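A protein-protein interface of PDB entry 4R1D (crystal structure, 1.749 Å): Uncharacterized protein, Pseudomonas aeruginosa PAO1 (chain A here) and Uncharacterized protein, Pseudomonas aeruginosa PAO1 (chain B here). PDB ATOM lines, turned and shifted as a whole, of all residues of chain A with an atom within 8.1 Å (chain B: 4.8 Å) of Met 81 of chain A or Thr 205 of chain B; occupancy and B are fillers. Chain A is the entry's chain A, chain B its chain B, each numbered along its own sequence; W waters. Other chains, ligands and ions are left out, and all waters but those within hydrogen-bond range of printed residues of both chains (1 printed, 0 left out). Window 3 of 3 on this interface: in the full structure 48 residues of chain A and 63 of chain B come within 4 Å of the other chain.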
ATOM      1  N   PRO A  75     -18.176  -3.313  23.598  1.00  0.00           N
ATOM      2  CA  PRO A  75     -18.796  -2.302  22.730  1.00  0.00           C
ATOM      3  C   PRO A  75     -20.312  -2.318  22.822  1.00  0.00           C
ATOM      4  O   PRO A  75     -20.904  -3.371  23.077  1.00  0.00           O
ATOM      5  CB  PRO A  75     -18.382  -2.765  21.331  1.00  0.00           C
ATOM      6  CG  PRO A  75     -18.330  -4.249  21.459  1.00  0.00           C
ATOM      7  CD  PRO A  75     -17.763  -4.505  22.838  1.00  0.00           C
ATOM      8  N   ASN A  76     -20.931  -1.160  22.594  1.00  0.00           N
ATOM      9  CA  ASN A  76     -22.387  -1.043  22.655  1.00  0.00           C
ATOM     10  C   ASN A  76     -22.979  -0.491  21.361  1.00  0.00           C
ATOM     11  O   ASN A  76     -24.159  -0.133  21.321  1.00  0.00           O
ATOM     12  CB  ASN A  76     -22.803  -0.145  23.830  1.00  0.00           C
ATOM     13  CG  ASN A  76     -22.387   1.306  23.632  1.00  0.00           C
ATOM     14  OD1 ASN A  76     -21.362   1.587  23.013  1.00  0.00           O
ATOM     15  ND2 ASN A  76     -23.181   2.230  24.152  1.00  0.00           N
ATOM     16  N   GLY A  77     -22.156  -0.401  20.316  1.00  0.00           N
ATOM     17  CA  GLY A  77     -22.590   0.171  19.050  1.00  0.00           C
ATOM     18  C   GLY A  77     -23.217  -0.841  18.101  1.00  0.00           C
ATOM     19  O   GLY A  77     -23.387  -2.009  18.447  1.00  0.00           O
ATOM     20  N   LEU A  78     -23.569  -0.391  16.900  1.00  0.00           N
ATOM     21  CA  LEU A  78     -24.117  -1.289  15.883  1.00  0.00           C
ATOM     22  C   LEU A  78     -22.979  -2.059  15.231  1.00  0.00           C
ATOM     23  O   LEU A  78     -23.199  -2.942  14.404  1.00  0.00           O
ATOM     24  CB  LEU A  78     -24.900  -0.507  14.827  1.00  0.00           C
ATOM     25  CG  LEU A  78     -26.042   0.350  15.374  1.00  0.00           C
ATOM     26  CD1 LEU A  78     -26.871   0.937  14.239  1.00  0.00           C
ATOM     27  CD2 LEU A  78     -26.918  -0.471  16.316  1.00  0.00           C
ATOM     28  N   TRP A  79     -21.759  -1.710  15.622  1.00  0.00           N
ATOM     29  CA  TRP A  79     -20.561  -2.342  15.099  1.00  0.00           C
ATOM     30  C   TRP A  79     -19.652  -2.730  16.260  1.00  0.00           C
ATOM     31  O   TRP A  79     -19.566  -2.007  17.249  1.00  0.00           O
ATOM     32  CB  TRP A  79     -19.837  -1.368  14.167  1.00  0.00           C
ATOM     33  CG  TRP A  79     -19.485  -1.955  12.842  1.00  0.00           C
ATOM     34  CD1 TRP A  79     -18.239  -2.303  12.403  1.00  0.00           C
ATOM     35  CD2 TRP A  79     -20.390  -2.273  11.776  1.00  0.00           C
ATOM     36  NE1 TRP A  79     -18.313  -2.817  11.128  1.00  0.00           N
ATOM     37  CE2 TRP A  79     -19.622  -2.809  10.721  1.00  0.00           C
ATOM     38  CE3 TRP A  79     -21.775  -2.155  11.612  1.00  0.00           C
ATOM     39  CZ2 TRP A  79     -20.194  -3.227   9.518  1.00  0.00           C
ATOM     40  CZ3 TRP A  79     -22.341  -2.571  10.418  1.00  0.00           C
ATOM     41  CH2 TRP A  79     -21.551  -3.101   9.386  1.00  0.00           C
ATOM     42  N   PRO A  80     -19.001  -3.898  16.168  1.00  0.00           N
ATOM     43  CA  PRO A  80     -19.247  -4.895  15.127  1.00  0.00           C
ATOM     44  C   PRO A  80     -20.194  -5.969  15.658  1.00  0.00           C
ATOM     45  O   PRO A  80     -19.843  -6.688  16.595  1.00  0.00           O
ATOM     46  CB  PRO A  80     -17.860  -5.490  14.904  1.00  0.00           C
ATOM     47  CG  PRO A  80     -17.232  -5.448  16.271  1.00  0.00           C
ATOM     48  CD  PRO A  80     -17.833  -4.254  16.998  1.00  0.00           C
ATOM     49  N   MET A  81     -21.388  -6.058  15.084  1.00  0.00           N
ATOM     50  CA  MET A  81     -22.317  -7.119  15.442  1.00  0.00           C
ATOM     51  C   MET A  81     -21.741  -8.450  14.976  1.00  0.00           C
ATOM     52  O   MET A  81     -22.238  -9.043  14.022  1.00  0.00           O
ATOM     53  CB  MET A  81     -23.675  -6.883  14.778  1.00  0.00           C
ATOM     54  CG  MET A  81     -24.448  -5.709  15.336  1.00  0.00           C
ATOM     55  SD  MET A  81     -25.139  -6.067  16.961  1.00  0.00           S
ATOM     56  CE  MET A  81     -26.498  -7.158  16.532  1.00  0.00           C
ATOM     57  N   ASP A  82     -20.690  -8.915  15.643  1.00  0.00           N
ATOM     58  CA  ASP A  82     -19.972 -10.102  15.189  1.00  0.00           C
ATOM     59  C   ASP A  82     -19.838 -11.157  16.280  1.00  0.00           C
ATOM     60  O   ASP A  82     -19.218 -12.199  16.074  1.00  0.00           O
ATOM     61  CB  ASP A  82     -18.582  -9.722  14.660  1.00  0.00           C
ATOM     62  CG  ASP A  82     -17.701  -9.080  15.726  1.00  0.00           C
ATOM     63  OD1 ASP A  82     -16.744  -8.368  15.357  1.00  0.00           O
ATOM     64  OD2 ASP A  82     -17.960  -9.282  16.932  1.00  0.00           O
ATOM     65  N   ASP A  83     -20.412 -10.881  17.444  1.00  0.00           N
ATOM     66  CA  ASP A  83     -20.324 -11.818  18.550  1.00  0.00           C
ATOM     67  C   ASP A  83     -21.603 -11.816  19.372  1.00  0.00           C
ATOM     68  O   ASP A  83     -22.022 -10.785  19.879  1.00  0.00           O
ATOM     69  CB  ASP A  83     -19.135 -11.484  19.446  1.00  0.00           C
ATOM     70  CG  ASP A  83     -18.967 -12.482  20.559  1.00  0.00           C
ATOM     71  OD1 ASP A  83     -18.552 -13.627  20.263  1.00  0.00           O
ATOM     72  OD2 ASP A  83     -19.266 -12.132  21.721  1.00  0.00           O
ATOM     73  N   LEU A  84     -22.219 -12.982  19.504  1.00  0.00           N
ATOM     74  CA  LEU A  84     -23.497 -13.080  20.205  1.00  0.00           C
ATOM     75  C   LEU A  84     -23.476 -12.506  21.628  1.00  0.00           C
ATOM     76  O   LEU A  84     -24.339 -11.708  21.995  1.00  0.00           O
ATOM     77  CB  LEU A  84     -23.964 -14.537  20.214  1.00  0.00           C
ATOM     78  CG  LEU A  84     -25.317 -14.820  20.849  1.00  0.00           C
ATOM     79  CD1 LEU A  84     -25.928 -16.042  20.182  1.00  0.00           C
ATOM     80  CD2 LEU A  84     -25.203 -15.001  22.365  1.00  0.00           C
ATOM     81  N   ALA A  86     -21.321 -10.498  23.049  1.00  0.00           N
ATOM     82  CA  ALA A  86     -21.034  -9.070  22.969  1.00  0.00           C
ATOM     83  C   ALA A  86     -22.333  -8.290  22.824  1.00  0.00           C
ATOM     84  O   ALA A  86     -22.530  -7.265  23.483  1.00  0.00           O
ATOM     85  CB  ALA A  86     -20.107  -8.780  21.788  1.00  0.00           C
ATOM     86  N   SER A  87     -23.219  -8.790  21.966  1.00  0.00           N
ATOM     87  CA  SER A  87     -24.483  -8.116  21.678  1.00  0.00           C
ATOM     88  C   SER A  87     -25.449  -8.202  22.872  1.00  0.00           C
ATOM     89  O   SER A  87     -26.205  -7.270  23.137  1.00  0.00           O
ATOM     90  CB  SER A  87     -25.112  -8.648  20.390  1.00  0.00           C
ATOM     91  OG  SER A  87     -25.788  -9.877  20.607  1.00  0.00           O
ATOM     92  N   ILE A  88     -25.409  -9.306  23.609  1.00  0.00           N
ATOM     93  CA  ILE A  88     -26.164  -9.378  24.864  1.00  0.00           C
ATOM     94  C   ILE A  88     -25.650  -8.318  25.836  1.00  0.00           C
ATOM     95  O   ILE A  88     -26.433  -7.619  26.483  1.00  0.00           O
ATOM     96  CB  ILE A  88     -26.120 -10.794  25.488  1.00  0.00           C
ATOM     97  CG1 ILE A  88     -26.972 -11.749  24.653  1.00  0.00           C
ATOM     98  CG2 ILE A  88     -26.603 -10.781  26.943  1.00  0.00           C
ATOM     99  CD1 ILE A  88     -26.999 -13.160  25.180  1.00  0.00           C
ATOM    100  N   ALA A  90     -24.345  -5.478  25.189  1.00  0.00           N
ATOM    101  CA  ALA A  90     -24.776  -4.155  24.753  1.00  0.00           C
ATOM    102  C   ALA A  90     -26.264  -3.967  24.994  1.00  0.00           C
ATOM    103  O   ALA A  90     -26.730  -2.872  25.315  1.00  0.00           O
ATOM    104  CB  ALA A  90     -24.447  -3.937  23.285  1.00  0.00           C
ATOM    105  N   GLN A 303     -18.099   1.772  17.409  1.00  0.00           N
ATOM    106  CA  GLN A 303     -18.218   0.612  18.291  1.00  0.00           C
ATOM    107  C   GLN A 303     -18.699   1.002  19.673  1.00  0.00           C
ATOM    108  O   GLN A 303     -19.387   0.226  20.347  1.00  0.00           O
ATOM    109  CB  GLN A 303     -16.868  -0.077  18.474  1.00  0.00           C
ATOM    110  CG  GLN A 303     -16.237  -0.609  17.235  1.00  0.00           C
ATOM    111  CD  GLN A 303     -15.087  -1.514  17.581  1.00  0.00           C
ATOM    112  OE1 GLN A 303     -15.249  -2.464  18.351  1.00  0.00           O
ATOM    113  NE2 GLN A 303     -13.909  -1.207  17.053  1.00  0.00           N
ATOM    114  N   PHE B 198     -32.759  -3.078  17.922  1.00  0.00           N
ATOM    115  CA  PHE B 198     -31.534  -3.761  18.315  1.00  0.00           C
ATOM    116  C   PHE B 198     -31.769  -5.265  18.424  1.00  0.00           C
ATOM    117  O   PHE B 198     -30.954  -6.063  17.956  1.00  0.00           O
ATOM    118  CB  PHE B 198     -30.974  -3.213  19.629  1.00  0.00           C
ATOM    119  CG  PHE B 198     -29.572  -3.672  19.917  1.00  0.00           C
ATOM    120  CD1 PHE B 198     -29.329  -4.672  20.845  1.00  0.00           C
ATOM    121  CD2 PHE B 198     -28.500  -3.126  19.230  1.00  0.00           C
ATOM    122  CE1 PHE B 198     -28.042  -5.101  21.101  1.00  0.00           C
ATOM    123  CE2 PHE B 198     -27.207  -3.553  19.479  1.00  0.00           C
ATOM    124  CZ  PHE B 198     -26.979  -4.542  20.422  1.00  0.00           C
ATOM    125  N   ASN B 201     -31.989  -6.855  15.140  1.00  0.00           N
ATOM    126  CA  ASN B 201     -30.622  -6.920  14.646  1.00  0.00           C
ATOM    127  C   ASN B 201     -29.906  -8.147  15.216  1.00  0.00           C
ATOM    128  O   ASN B 201     -29.234  -8.885  14.494  1.00  0.00           O
ATOM    129  CB  ASN B 201     -29.862  -5.637  15.001  1.00  0.00           C
ATOM    130  CG  ASN B 201     -28.547  -5.511  14.263  1.00  0.00           C
ATOM    131  OD1 ASN B 201     -28.027  -6.487  13.720  1.00  0.00           O
ATOM    132  ND2 ASN B 201     -27.996  -4.298  14.240  1.00  0.00           N
ATOM    133  N   MET B 202     -30.066  -8.377  16.515  1.00  0.00           N
ATOM    134  CA  MET B 202     -29.463  -9.544  17.141  1.00  0.00           C
ATOM    135  C   MET B 202     -30.003 -10.844  16.535  1.00  0.00           C
ATOM    136  O   MET B 202     -29.233 -11.771  16.258  1.00  0.00           O
ATOM    137  CB  MET B 202     -29.704  -9.538  18.655  1.00  0.00           C
ATOM    138  CG  MET B 202     -29.098  -8.363  19.406  1.00  0.00           C
ATOM    139  SD  MET B 202     -29.665  -8.354  21.132  1.00  0.00           S
ATOM    140  CE  MET B 202     -28.730  -9.721  21.829  1.00  0.00           C
ATOM    141  N   LEU B 203     -31.318 -10.920  16.346  1.00  0.00           N
ATOM    142  CA  LEU B 203     -31.940 -12.142  15.833  1.00  0.00           C
ATOM    143  C   LEU B 203     -31.479 -12.423  14.412  1.00  0.00           C
ATOM    144  O   LEU B 203     -31.264 -13.574  14.025  1.00  0.00           O
ATOM    145  CB  LEU B 203     -33.461 -12.026  15.844  1.00  0.00           C
ATOM    146  CG  LEU B 203     -34.131 -11.930  17.213  1.00  0.00           C
ATOM    147  CD1 LEU B 203     -35.613 -11.629  17.046  1.00  0.00           C
ATOM    148  CD2 LEU B 203     -33.918 -13.212  18.003  1.00  0.00           C
ATOM    149  N   SER B 204     -31.346 -11.354  13.637  1.00  0.00           N
ATOM    150  CA  SER B 204     -30.988 -11.461  12.232  1.00  0.00           C
ATOM    151  C   SER B 204     -29.537 -11.873  12.069  1.00  0.00           C
ATOM    152  O   SER B 204     -29.187 -12.590  11.128  1.00  0.00           O
ATOM    153  CB  SER B 204     -31.235 -10.124  11.516  1.00  0.00           C
ATOM    154  OG  SER B 204     -32.622  -9.858  11.398  1.00  0.00           O
ATOM    155  N   THR B 205     -28.696 -11.410  12.988  1.00  0.00           N
ATOM    156  CA  THR B 205     -27.263 -11.632  12.902  1.00  0.00           C
ATOM    157  C   THR B 205     -26.844 -12.971  13.503  1.00  0.00           C
ATOM    158  O   THR B 205     -25.917 -13.615  13.008  1.00  0.00           O
ATOM    159  CB  THR B 205     -26.490 -10.509  13.611  1.00  0.00           C
ATOM    160  OG1 THR B 205     -26.876  -9.242  13.061  1.00  0.00           O
ATOM    161  CG2 THR B 205     -24.998 -10.702  13.441  1.00  0.00           C
ATOM    162  N   PHE B 206     -27.526 -13.380  14.570  1.00  0.00           N
ATOM    163  CA  PHE B 206     -27.114 -14.556  15.340  1.00  0.00           C
ATOM    164  C   PHE B 206     -28.189 -15.640  15.383  1.00  0.00           C
ATOM    165  O   PHE B 206     -29.232 -15.467  16.010  1.00  0.00           O
ATOM    166  CB  PHE B 206     -26.728 -14.153  16.771  1.00  0.00           C
ATOM    167  CG  PHE B 206     -25.677 -13.075  16.837  1.00  0.00           C
ATOM    168  CD1 PHE B 206     -24.354 -13.357  16.530  1.00  0.00           C
ATOM    169  CD2 PHE B 206     -26.013 -11.778  17.203  1.00  0.00           C
ATOM    170  CE1 PHE B 206     -23.384 -12.370  16.583  1.00  0.00           C
ATOM    171  CE2 PHE B 206     -25.047 -10.786  17.266  1.00  0.00           C
ATOM    172  CZ  PHE B 206     -23.731 -11.081  16.951  1.00  0.00           C
ATOM    173  N   ALA B 207     -27.926 -16.768  14.729  1.00  0.00           N
ATOM    174  CA  ALA B 207     -28.890 -17.864  14.704  1.00  0.00           C
ATOM    175  C   ALA B 207     -29.126 -18.411  16.106  1.00  0.00           C
ATOM    176  O   ALA B 207     -30.173 -18.995  16.384  1.00  0.00           O
ATOM    177  CB  ALA B 207     -28.405 -18.976  13.776  1.00  0.00           C
HETATM  178  O   HOH W   1     -25.419  -3.663  12.793  1.00  0.00           O
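OD1 of Asn 201 of chain B touches CE of Met 81 of chain A, 3.3 Å away.
Met 81 of chain A touches Thr 205 of chain B (O to CG2, 3.3 Å).
CZ of Phe 206 of chain B touches C of Met 81 of chain A, at 3.8 Å.
Asp 82 of chain A touches Phe 206 of chain B.
Phe 206 of chain B touches Asp 83 of chain A (CZ to C, 3.3 Å).
Ser 87 of chain A touches Phe 198 of chain B.
CE of Met 202 of chain B touches OG of Ser 87 of chain A, 3.2 Å away.
OG of Ser 87 of chain A touches CE2 of Phe 206 of chain B (3.5 Å).
Ile 88 of chain A touches Met 202 of chain B (N to CE, 3.8 Å).
CB of Ala 90 of chain A touches CZ of Phe 198 of chain B (3.9 Å).
Water W1 lies within hydrogen-bond range of the backbone carbonyl oxygen (O) of Leu 78 of chain A (2.8 Å) and the side-chain amide nitrogen (ND2) of Asn 201 of chain B (3.0 Å).
Of chain B, only Asn 201, Met 202, Thr 205 and Phe 206 come within 4 Å of Met 81 of chain A.
Of the printed residues of chain B, Ala 90 of chain A touches Phe 198.
Of the printed residues of chain A, Met 202 of chain B touches Met 81 (3.8 Å), Ser 87 (3.2 Å) and Ile 88 (3.8 Å).
Asn 76 of chain A touches none of the printed residues of chain B.
Leu 203 of chain B touches none of the printed residues of chain A.
The nearest residue of chain A that does not touch Thr 205 of chain B is Asp 82 of chain A (5.2 Å).
The side-chain carboxylate (OD2) of Asp 83 of chain A sits at hydrogen-bond distance from the backbone NH (N) of Ala 86 of chain A.
The backbone carbonyl oxygen of Leu 84 of chain A sits at hydrogen-bond distance from the side-chain hydroxyl of Ser 87 of chain A, at 2.7 Å.
The backbone carbonyl oxygen (O) of Asn 201 of chain B is in hydrogen-bond range of the side-chain hydroxyl (OG1) of Thr 205 of chain B (2.8 Å).
Of the 15 printed residues of chain A, 7 touch a printed residue of chain B.
Printed residues of chain A that touch a printed residue of chain B: Met 81, Asp 82, Asp 83, Leu 84, Ser 87, Ile 88 and Ala 90.
Hydrophobic or aromatic side chains of chain A within 4 Å of the printed part of chain B: Met 81, Leu 84, Ile 88 and Ala 90.
Along chain B the printed residues that touch a printed residue of chain A span positions 198 to 206.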
